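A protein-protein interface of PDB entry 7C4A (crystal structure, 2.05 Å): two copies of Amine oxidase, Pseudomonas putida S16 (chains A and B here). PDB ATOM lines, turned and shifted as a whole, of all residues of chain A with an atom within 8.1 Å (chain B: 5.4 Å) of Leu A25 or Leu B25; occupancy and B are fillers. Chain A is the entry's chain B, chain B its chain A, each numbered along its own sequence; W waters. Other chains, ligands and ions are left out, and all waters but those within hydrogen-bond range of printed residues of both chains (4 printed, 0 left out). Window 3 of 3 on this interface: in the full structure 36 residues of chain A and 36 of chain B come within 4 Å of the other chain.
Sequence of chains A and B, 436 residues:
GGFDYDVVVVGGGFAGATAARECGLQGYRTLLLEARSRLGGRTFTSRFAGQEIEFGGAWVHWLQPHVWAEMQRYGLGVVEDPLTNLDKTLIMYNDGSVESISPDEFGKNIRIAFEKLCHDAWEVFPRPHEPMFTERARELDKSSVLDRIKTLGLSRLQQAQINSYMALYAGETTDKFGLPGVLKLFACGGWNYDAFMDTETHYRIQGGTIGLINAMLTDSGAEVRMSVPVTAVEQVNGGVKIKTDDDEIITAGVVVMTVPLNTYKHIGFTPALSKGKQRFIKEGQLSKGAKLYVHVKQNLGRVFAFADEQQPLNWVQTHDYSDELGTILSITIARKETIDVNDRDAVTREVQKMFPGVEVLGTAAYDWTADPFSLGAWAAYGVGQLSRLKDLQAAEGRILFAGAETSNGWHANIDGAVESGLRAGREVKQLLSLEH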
ATOM      1  N   THR A  18     -11.470   4.657 -17.085  1.00  0.00           N
ATOM      2  CA  THR A  18     -12.188   5.904 -17.138  1.00  0.00           C
ATOM      3  C   THR A  18     -13.662   5.709 -16.777  1.00  0.00           C
ATOM      4  O   THR A  18     -14.167   6.425 -15.955  1.00  0.00           O
ATOM      5  CB  THR A  18     -12.015   6.606 -18.508  1.00  0.00           C
ATOM      6  OG1 THR A  18     -10.612   6.840 -18.712  1.00  0.00           O
ATOM      7  CG2 THR A  18     -12.776   7.930 -18.535  1.00  0.00           C
ATOM      8  N   ALA A  19     -14.313   4.723 -17.378  1.00  0.00           N
ATOM      9  CA  ALA A  19     -15.708   4.455 -17.110  1.00  0.00           C
ATOM     10  C   ALA A  19     -15.912   4.047 -15.651  1.00  0.00           C
ATOM     11  O   ALA A  19     -16.844   4.491 -15.007  1.00  0.00           O
ATOM     12  CB  ALA A  19     -16.260   3.389 -18.048  1.00  0.00           C
ATOM     13  N   ALA A  20     -15.018   3.233 -15.105  1.00  0.00           N
ATOM     14  CA  ALA A  20     -15.114   2.821 -13.703  1.00  0.00           C
ATOM     15  C   ALA A  20     -14.976   4.016 -12.719  1.00  0.00           C
ATOM     16  O   ALA A  20     -15.687   4.083 -11.718  1.00  0.00           O
ATOM     17  CB  ALA A  20     -14.079   1.743 -13.373  1.00  0.00           C
ATOM     18  N   ARG A  21     -14.092   4.950 -13.053  1.00  0.00           N
ATOM     19  CA  ARG A  21     -13.843   6.158 -12.251  1.00  0.00           C
ATOM     20  C   ARG A  21     -15.110   7.056 -12.293  1.00  0.00           C
ATOM     21  O   ARG A  21     -15.617   7.492 -11.254  1.00  0.00           O
ATOM     22  CB  ARG A  21     -12.633   6.905 -12.808  1.00  0.00           C
ATOM     23  CG  ARG A  21     -12.047   8.006 -11.912  1.00  0.00           C
ATOM     24  CD  ARG A  21     -12.807   9.329 -11.953  1.00  0.00           C
ATOM     25  NE  ARG A  21     -13.054   9.785 -13.326  1.00  0.00           N
ATOM     26  CZ  ARG A  21     -12.128  10.291 -14.150  1.00  0.00           C
ATOM     27  NH1 ARG A  21     -10.861  10.449 -13.762  1.00  0.00           N
ATOM     28  NH2 ARG A  21     -12.494  10.666 -15.378  1.00  0.00           N
ATOM     29  N   GLU A  22     -15.686   7.211 -13.484  1.00  0.00           N
ATOM     30  CA  GLU A  22     -16.927   8.015 -13.638  1.00  0.00           C
ATOM     31  C   GLU A  22     -18.045   7.394 -12.783  1.00  0.00           C
ATOM     32  O   GLU A  22     -18.677   8.126 -12.021  1.00  0.00           O
ATOM     33  CB  GLU A  22     -17.309   8.126 -15.116  1.00  0.00           C
ATOM     34  CG  GLU A  22     -16.340   8.963 -15.930  1.00  0.00           C
ATOM     35  CD  GLU A  22     -16.289  10.435 -15.553  1.00  0.00           C
ATOM     36  OE1 GLU A  22     -17.279  11.136 -15.793  1.00  0.00           O
ATOM     37  OE2 GLU A  22     -15.276  10.861 -15.000  1.00  0.00           O
ATOM     38  N   CYS A  23     -18.224   6.078 -12.864  1.00  0.00           N
ATOM     39  CA  CYS A  23     -19.309   5.376 -12.127  1.00  0.00           C
ATOM     40  C   CYS A  23     -19.058   5.375 -10.610  1.00  0.00           C
ATOM     41  O   CYS A  23     -19.991   5.653  -9.856  1.00  0.00           O
ATOM     42  CB  CYS A  23     -19.449   3.959 -12.661  1.00  0.00           C
ATOM     43  SG  CYS A  23     -20.052   3.903 -14.368  1.00  0.00           S
ATOM     44  N   GLY A  24     -17.823   5.108 -10.198  1.00  0.00           N
ATOM     45  CA  GLY A  24     -17.465   5.015  -8.799  1.00  0.00           C
ATOM     46  C   GLY A  24     -17.677   6.302  -8.064  1.00  0.00           C
ATOM     47  O   GLY A  24     -18.204   6.309  -6.935  1.00  0.00           O
ATOM     48  N   LEU A  25     -17.345   7.418  -8.724  1.00  0.00           N
ATOM     49  CA  LEU A  25     -17.481   8.712  -8.062  1.00  0.00           C
ATOM     50  C   LEU A  25     -18.953   9.164  -7.966  1.00  0.00           C
ATOM     51  O   LEU A  25     -19.268  10.046  -7.195  1.00  0.00           O
ATOM     52  CB  LEU A  25     -16.635   9.783  -8.737  1.00  0.00           C
ATOM     53  CG  LEU A  25     -15.110   9.586  -8.643  1.00  0.00           C
ATOM     54  CD1 LEU A  25     -14.462  10.863  -9.144  1.00  0.00           C
ATOM     55  CD2 LEU A  25     -14.679   9.278  -7.246  1.00  0.00           C
ATOM     56  N   GLN A  26     -19.852   8.528  -8.721  1.00  0.00           N
ATOM     57  CA  GLN A  26     -21.293   8.773  -8.549  1.00  0.00           C
ATOM     58  C   GLN A  26     -21.848   8.011  -7.343  1.00  0.00           C
ATOM     59  O   GLN A  26     -23.002   8.186  -6.964  1.00  0.00           O
ATOM     60  CB  GLN A  26     -22.081   8.376  -9.800  1.00  0.00           C
ATOM     61  CG  GLN A  26     -21.797   9.210 -11.012  1.00  0.00           C
ATOM     62  CD  GLN A  26     -22.156  10.678 -10.797  1.00  0.00           C
ATOM     63  OE1 GLN A  26     -23.262  11.002 -10.379  1.00  0.00           O
ATOM     64  NE2 GLN A  26     -21.220  11.567 -11.109  1.00  0.00           N
ATOM     65  N   GLY A  27     -21.038   7.135  -6.745  1.00  0.00           N
ATOM     66  CA  GLY A  27     -21.504   6.313  -5.638  1.00  0.00           C
ATOM     67  C   GLY A  27     -22.122   4.980  -6.055  1.00  0.00           C
ATOM     68  O   GLY A  27     -22.709   4.288  -5.224  1.00  0.00           O
ATOM     69  N   TYR A  28     -22.009   4.617  -7.338  1.00  0.00           N
ATOM     70  CA  TYR A  28     -22.532   3.338  -7.797  1.00  0.00           C
ATOM     71  C   TYR A  28     -21.583   2.209  -7.306  1.00  0.00           C
ATOM     72  O   TYR A  28     -20.342   2.390  -7.273  1.00  0.00           O
ATOM     73  CB  TYR A  28     -22.661   3.289  -9.312  1.00  0.00           C
ATOM     74  CG  TYR A  28     -23.491   4.383  -9.939  1.00  0.00           C
ATOM     75  CD1 TYR A  28     -24.632   4.852  -9.340  1.00  0.00           C
ATOM     76  CD2 TYR A  28     -23.104   4.943 -11.140  1.00  0.00           C
ATOM     77  CE1 TYR A  28     -25.411   5.857  -9.917  1.00  0.00           C
ATOM     78  CE2 TYR A  28     -23.853   5.938 -11.729  1.00  0.00           C
ATOM     79  CZ  TYR A  28     -25.003   6.394 -11.108  1.00  0.00           C
ATOM     80  OH  TYR A  28     -25.735   7.393 -11.679  1.00  0.00           O
ATOM     81  N   THR A  30     -19.507  -0.504  -8.054  1.00  0.00           N
ATOM     82  CA  THR A  30     -18.841  -0.714  -9.345  1.00  0.00           C
ATOM     83  C   THR A  30     -17.806  -1.837  -9.269  1.00  0.00           C
ATOM     84  O   THR A  30     -16.983  -1.909  -8.334  1.00  0.00           O
ATOM     85  CB  THR A  30     -18.154   0.592  -9.789  1.00  0.00           C
ATOM     86  OG1 THR A  30     -19.117   1.643  -9.779  1.00  0.00           O
ATOM     87  CG2 THR A  30     -17.557   0.483 -11.179  1.00  0.00           C
ATOM     88  N   ARG A  73      -6.096  16.653 -13.636  1.00  0.00           N
ATOM     89  CA  ARG A  73      -6.824  16.156 -12.455  1.00  0.00           C
ATOM     90  C   ARG A  73      -5.902  15.430 -11.500  1.00  0.00           C
ATOM     91  O   ARG A  73      -6.003  15.629 -10.311  1.00  0.00           O
ATOM     92  CB  ARG A  73      -7.966  15.223 -12.856  1.00  0.00           C
ATOM     93  CG  ARG A  73      -8.674  14.500 -11.710  1.00  0.00           C
ATOM     94  CD  ARG A  73      -9.903  13.692 -12.216  1.00  0.00           C
ATOM     95  NE  ARG A  73     -11.016  14.598 -12.476  1.00  0.00           N
ATOM     96  CZ  ARG A  73     -11.499  14.948 -13.671  1.00  0.00           C
ATOM     97  NH1 ARG A  73     -11.042  14.436 -14.787  1.00  0.00           N
ATOM     98  NH2 ARG A  73     -12.490  15.832 -13.760  1.00  0.00           N
ATOM     99  N   TYR A  74      -5.038  14.552 -12.031  1.00  0.00           N
ATOM    100  CA  TYR A  74      -4.157  13.745 -11.196  1.00  0.00           C
ATOM    101  C   TYR A  74      -2.762  14.304 -11.006  1.00  0.00           C
ATOM    102  O   TYR A  74      -1.975  13.719 -10.313  1.00  0.00           O
ATOM    103  CB  TYR A  74      -4.145  12.288 -11.685  1.00  0.00           C
ATOM    104  CG  TYR A  74      -5.507  11.681 -11.554  1.00  0.00           C
ATOM    105  CD1 TYR A  74      -6.047  11.392 -10.295  1.00  0.00           C
ATOM    106  CD2 TYR A  74      -6.274  11.442 -12.678  1.00  0.00           C
ATOM    107  CE1 TYR A  74      -7.325  10.849 -10.188  1.00  0.00           C
ATOM    108  CE2 TYR A  74      -7.569  10.907 -12.591  1.00  0.00           C
ATOM    109  CZ  TYR A  74      -8.091  10.632 -11.347  1.00  0.00           C
ATOM    110  OH  TYR A  74      -9.349  10.095 -11.267  1.00  0.00           O
ATOM    111  N   MET A 216      -6.801   6.520 -11.566  1.00  0.00           N
ATOM    112  CA  MET A 216      -8.233   6.504 -11.835  1.00  0.00           C
ATOM    113  C   MET A 216      -8.953   5.389 -11.081  1.00  0.00           C
ATOM    114  O   MET A 216      -9.984   5.639 -10.454  1.00  0.00           O
ATOM    115  CB  MET A 216      -8.486   6.410 -13.332  1.00  0.00           C
ATOM    116  CG  MET A 216      -8.151   7.691 -14.060  1.00  0.00           C
ATOM    117  SD  MET A 216      -8.697   7.503 -15.973  1.00  0.00           S
ATOM    118  CE  MET A 216      -9.834   8.998 -16.348  1.00  0.00           C
ATOM    119  N   LEU A 217      -8.375   4.178 -11.070  1.00  0.00           N
ATOM    120  CA  LEU A 217      -8.980   3.074 -10.339  1.00  0.00           C
ATOM    121  C   LEU A 217      -8.989   3.232  -8.851  1.00  0.00           C
ATOM    122  O   LEU A 217      -9.966   2.902  -8.234  1.00  0.00           O
ATOM    123  CB  LEU A 217      -8.356   1.743 -10.753  1.00  0.00           C
ATOM    124  CG  LEU A 217      -8.753   1.390 -12.188  1.00  0.00           C
ATOM    125  CD1 LEU A 217      -7.936   0.203 -12.614  1.00  0.00           C
ATOM    126  CD2 LEU A 217     -10.236   1.119 -12.318  1.00  0.00           C
ATOM    127  N   THR A 218      -7.883   3.720  -8.281  1.00  0.00           N
ATOM    128  CA  THR A 218      -7.815   4.090  -6.895  1.00  0.00           C
ATOM    129  C   THR A 218      -8.891   5.157  -6.526  1.00  0.00           C
ATOM    130  O   THR A 218      -9.603   5.007  -5.547  1.00  0.00           O
ATOM    131  CB  THR A 218      -6.397   4.522  -6.523  1.00  0.00           C
ATOM    132  OG1 THR A 218      -5.566   3.360  -6.583  1.00  0.00           O
ATOM    133  CG2 THR A 218      -6.309   5.078  -5.091  1.00  0.00           C
ATOM    134  N   ASP A 219      -8.984   6.221  -7.334  1.00  0.00           N
ATOM    135  CA  ASP A 219      -9.991   7.262  -7.181  1.00  0.00           C
ATOM    136  C   ASP A 219     -11.417   6.649  -7.215  1.00  0.00           C
ATOM    137  O   ASP A 219     -12.275   7.014  -6.403  1.00  0.00           O
ATOM    138  CB  ASP A 219      -9.832   8.305  -8.314  1.00  0.00           C
ATOM    139  CG  ASP A 219     -10.486   9.650  -8.014  1.00  0.00           C
ATOM    140  OD1 ASP A 219     -10.953   9.880  -6.862  1.00  0.00           O
ATOM    141  OD2 ASP A 219     -10.511  10.484  -8.964  1.00  0.00           O
ATOM    142  N   SER A 220     -11.638   5.688  -8.114  1.00  0.00           N
ATOM    143  CA  SER A 220     -12.972   5.152  -8.372  1.00  0.00           C
ATOM    144  C   SER A 220     -13.615   4.486  -7.148  1.00  0.00           C
ATOM    145  O   SER A 220     -14.831   4.483  -7.019  1.00  0.00           O
ATOM    146  CB  SER A 220     -12.950   4.129  -9.510  1.00  0.00           C
ATOM    147  OG  SER A 220     -12.399   2.857  -9.135  1.00  0.00           O
ATOM    148  N   GLY A 221     -12.801   3.853  -6.307  1.00  0.00           N
ATOM    149  CA  GLY A 221     -13.285   2.969  -5.265  1.00  0.00           C
ATOM    150  C   GLY A 221     -13.834   1.621  -5.831  1.00  0.00           C
ATOM    151  O   GLY A 221     -14.367   0.831  -5.084  1.00  0.00           O
ATOM    152  N   ALA A 222     -13.714   1.368  -7.137  1.00  0.00           N
ATOM    153  CA  ALA A 222     -14.311   0.174  -7.693  1.00  0.00           C
ATOM    154  C   ALA A 222     -13.545  -1.077  -7.251  1.00  0.00           C
ATOM    155  O   ALA A 222     -12.328  -1.043  -7.046  1.00  0.00           O
ATOM    156  CB  ALA A 222     -14.348   0.245  -9.206  1.00  0.00           C
ATOM    157  N   LYS A 429     -25.121   6.756 -15.958  1.00  0.00           N
ATOM    158  CA  LYS A 429     -25.848   7.675 -15.099  1.00  0.00           C
ATOM    159  C   LYS A 429     -27.301   7.908 -15.577  1.00  0.00           C
ATOM    160  O   LYS A 429     -28.245   7.920 -14.764  1.00  0.00           O
ATOM    161  CB  LYS A 429     -25.051   8.969 -14.943  1.00  0.00           C
ATOM    162  CG  LYS A 429     -25.759   9.996 -14.094  1.00  0.00           C
ATOM    163  CD  LYS A 429     -24.816  11.138 -13.670  1.00  0.00           C
ATOM    164  CE  LYS A 429     -25.547  12.093 -12.709  1.00  0.00           C
ATOM    165  NZ  LYS A 429     -24.685  13.238 -12.302  1.00  0.00           N
ATOM    166  N   ALA B  20     -15.981  22.750  -6.985  1.00  0.00           N
ATOM    167  CA  ALA B  20     -17.059  22.177  -6.141  1.00  0.00           C
ATOM    168  C   ALA B  20     -17.454  20.758  -6.596  1.00  0.00           C
ATOM    169  O   ALA B  20     -17.732  19.888  -5.770  1.00  0.00           O
ATOM    170  CB  ALA B  20     -18.292  23.067  -6.120  1.00  0.00           C
ATOM    171  N   ARG B  21     -17.459  20.549  -7.910  1.00  0.00           N
ATOM    172  CA  ARG B  21     -17.790  19.263  -8.520  1.00  0.00           C
ATOM    173  C   ARG B  21     -16.714  18.216  -8.150  1.00  0.00           C
ATOM    174  O   ARG B  21     -17.031  17.113  -7.691  1.00  0.00           O
ATOM    175  CB  ARG B  21     -17.937  19.435 -10.034  1.00  0.00           C
ATOM    176  CG  ARG B  21     -18.574  18.288 -10.800  1.00  0.00           C
ATOM    177  CD  ARG B  21     -17.663  17.108 -11.042  1.00  0.00           C
ATOM    178  NE  ARG B  21     -16.393  17.465 -11.643  1.00  0.00           N
ATOM    179  CZ  ARG B  21     -16.208  17.878 -12.904  1.00  0.00           C
ATOM    180  NH1 ARG B  21     -17.218  17.971 -13.770  1.00  0.00           N
ATOM    181  NH2 ARG B  21     -14.979  18.194 -13.323  1.00  0.00           N
ATOM    182  N   GLU B  22     -15.440  18.584  -8.293  1.00  0.00           N
ATOM    183  CA  GLU B  22     -14.358  17.703  -7.865  1.00  0.00           C
ATOM    184  C   GLU B  22     -14.453  17.269  -6.391  1.00  0.00           C
ATOM    185  O   GLU B  22     -14.271  16.088  -6.055  1.00  0.00           O
ATOM    186  CB  GLU B  22     -12.982  18.319  -8.145  1.00  0.00           C
ATOM    187  CG  GLU B  22     -12.675  18.594  -9.635  1.00  0.00           C
ATOM    188  CD  GLU B  22     -12.562  17.309 -10.451  1.00  0.00           C
ATOM    189  OE1 GLU B  22     -11.510  16.582 -10.314  1.00  0.00           O
ATOM    190  OE2 GLU B  22     -13.534  16.979 -11.201  1.00  0.00           O
ATOM    191  N   CYS B  23     -14.663  18.253  -5.511  1.00  0.00           N
ATOM    192  CA  CYS B  23     -14.786  18.027  -4.082  1.00  0.00           C
ATOM    193  C   CYS B  23     -16.017  17.204  -3.712  1.00  0.00           C
ATOM    194  O   CYS B  23     -15.953  16.230  -2.916  1.00  0.00           O
ATOM    195  CB  CYS B  23     -14.795  19.397  -3.371  1.00  0.00           C
ATOM    196  SG  CYS B  23     -13.182  20.206  -3.505  1.00  0.00           S
ATOM    197  N   GLY B  24     -17.159  17.572  -4.296  1.00  0.00           N
ATOM    198  CA  GLY B  24     -18.382  16.879  -3.971  1.00  0.00           C
ATOM    199  C   GLY B  24     -18.373  15.419  -4.342  1.00  0.00           C
ATOM    200  O   GLY B  24     -18.854  14.579  -3.597  1.00  0.00           O
ATOM    201  N   LEU B  25     -17.788  15.105  -5.495  1.00  0.00           N
ATOM    202  CA  LEU B  25     -17.723  13.712  -5.959  1.00  0.00           C
ATOM    203  C   LEU B  25     -16.728  12.873  -5.144  1.00  0.00           C
ATOM    204  O   LEU B  25     -16.822  11.678  -5.179  1.00  0.00           O
ATOM    205  CB  LEU B  25     -17.398  13.612  -7.448  1.00  0.00           C
ATOM    206  CG  LEU B  25     -18.470  14.141  -8.392  1.00  0.00           C
ATOM    207  CD1 LEU B  25     -18.101  13.736  -9.814  1.00  0.00           C
ATOM    208  CD2 LEU B  25     -19.861  13.699  -8.026  1.00  0.00           C
ATOM    209  N   GLN B  26     -15.829  13.520  -4.382  1.00  0.00           N
ATOM    210  CA  GLN B  26     -14.967  12.797  -3.458  1.00  0.00           C
ATOM    211  C   GLN B  26     -15.724  12.437  -2.167  1.00  0.00           C
ATOM    212  O   GLN B  26     -15.222  11.705  -1.342  1.00  0.00           O
ATOM    213  CB  GLN B  26     -13.718  13.601  -3.124  1.00  0.00           C
ATOM    214  CG  GLN B  26     -12.740  13.809  -4.282  1.00  0.00           C
ATOM    215  CD  GLN B  26     -12.214  12.476  -4.814  1.00  0.00           C
ATOM    216  OE1 GLN B  26     -11.716  11.653  -4.043  1.00  0.00           O
ATOM    217  NE2 GLN B  26     -12.359  12.243  -6.128  1.00  0.00           N
ATOM    218  N   GLY B  27     -16.936  12.973  -1.993  1.00  0.00           N
ATOM    219  CA  GLY B  27     -17.685  12.749  -0.768  1.00  0.00           C
ATOM    220  C   GLY B  27     -17.475  13.808   0.300  1.00  0.00           C
ATOM    221  O   GLY B  27     -17.963  13.646   1.392  1.00  0.00           O
ATOM    222  N   ASP B 219     -24.328  17.797 -10.299  1.00  0.00           N
ATOM    223  CA  ASP B 219     -23.477  16.612 -10.135  1.00  0.00           C
ATOM    224  C   ASP B 219     -22.762  16.644  -8.770  1.00  0.00           C
ATOM    225  O   ASP B 219     -22.697  15.635  -8.072  1.00  0.00           O
ATOM    226  CB  ASP B 219     -22.442  16.576 -11.276  1.00  0.00           C
ATOM    227  CG  ASP B 219     -21.807  15.201 -11.495  1.00  0.00           C
ATOM    228  OD1 ASP B 219     -22.326  14.199 -10.912  1.00  0.00           O
ATOM    229  OD2 ASP B 219     -20.830  15.159 -12.309  1.00  0.00           O
ATOM    230  N   SER B 220     -22.273  17.824  -8.360  1.00  0.00           N
ATOM    231  CA  SER B 220     -21.431  17.933  -7.173  1.00  0.00           C
ATOM    232  C   SER B 220     -22.117  17.476  -5.870  1.00  0.00           C
ATOM    233  O   SER B 220     -21.455  17.040  -4.949  1.00  0.00           O
ATOM    234  CB  SER B 220     -20.959  19.375  -6.961  1.00  0.00           C
ATOM    235  OG  SER B 220     -21.962  20.254  -6.448  1.00  0.00           O
HETATM  236  O   HOH W   1     -12.155   8.928  -4.371  1.00  0.00           O
HETATM  237  O   HOH W   2     -19.727  13.173 -13.446  1.00  0.00           O
HETATM  238  O   HOH W   3     -23.596  13.018  -8.541  1.00  0.00           O
HETATM  239  O   HOH W   4     -10.860  12.928  -8.930  1.00  0.00           O
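The side-chain carboxylate of Glu B22 lies within salt-bridge range of the guanidinium group of Arg A73, at 3.0 Å. The side-chain amide nitrogen (NE2) of Gln B26 lies within hydrogen-bond range of the side-chain carboxylate (OD1) of Asp A219. OD1 of Asp B219 is in hydrogen-bond range of NE2 of Gln A26 (2.9 Å). The side-chain amino group of Lys A429 is in salt-bridge range of the side-chain carboxylate of Asp B219 (2.9 Å). The guanidinium group (NH2) of Arg A73 lies close to the guanidinium group (NH2) of Arg B21 (3.5 Å).
NH2 of Arg B21 lies within salt-bridge range of OE2 of Glu B22 (2.8 Å). OE1 of Gln A26 sits at hydrogen-bond distance from NZ of Lys A429 (3.3 Å). OH of Tyr A74 lies within hydrogen-bond range of OD2 of Asp A219, at 2.6 Å.
Among the printed residues, pairs that only touch across the chains: Leu A25 with Leu B25, Leu A25 with Gln B26 and Gln A26 with Leu B25.
Glu A22 touches none of the printed residues of chain B. Of chain B, only Leu B25 (3.6 Å) and Gln B26 (3.9 Å) come within 4 Å of Leu A25. Of the printed residues of chain B, Arg A73 touches Arg B21 and Glu B22. Printed residues of chain B within 4 Å of Asp A219: Gln B26 (2.8 Å). Printed residues of chain B within 4 Å of Lys A429: Asp B219. Of the printed residues of chain A, Glu B22 touches Arg A73 (3.0 Å). No residue of chain A comes within 4 Å of Gly B24. Of the printed residues of chain A, Leu B25 touches Leu A25 (3.6 Å) and Gln A26 (3.99 Å). Of the printed residues of chain A, Gln B26 touches Leu A25 and Asp A219.
Hydrophobic or aromatic side chains of chain B that line the printed part of chain A: Leu B25. Along chain B the printed residues that touch a printed residue of chain A span positions 21 to 219. Among the printed residues, Asp or Glu carboxylates within 4 Å of a Lys or Arg side-chain nitrogen of the other chain: Arg A73 with Glu B22 (3.0 Å) and Lys A429 with Asp B219 (2.9 Å).
Leu A25 touches its own counterpart, Leu B25. Leu A25 touches Gln B26, and with the chains exchanged Gln A26 touches Leu B25. Gln A26 touches Asp B219, and with the chains exchanged Asp A219 touches Gln B26. Of the 8 pairs that touch across the chains among the printed residues, 5 have their exchanged pair printed and touching as well.
Water W4 bridges OD2 of Asp A219 (2.5 Å) and NE2 of Gln B26 (3.3 Å). Water W2 lies within hydrogen-bond range of the side-chain carboxylate (OD2) of Asp B219 (2.5 Å) and the side-chain amide nitrogen (NE2) of Gln A26 (3.2 Å). Water W3 lies within hydrogen-bond range of the side-chain amide oxygen of Gln A26 (2.7 Å) and the backbone carbonyl oxygen of Asp B219 (2.8 Å). Water W1 lies within hydrogen-bond range of OE1 of Gln B26 (2.8 Å) and O of Asp A219 (2.8 Å).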
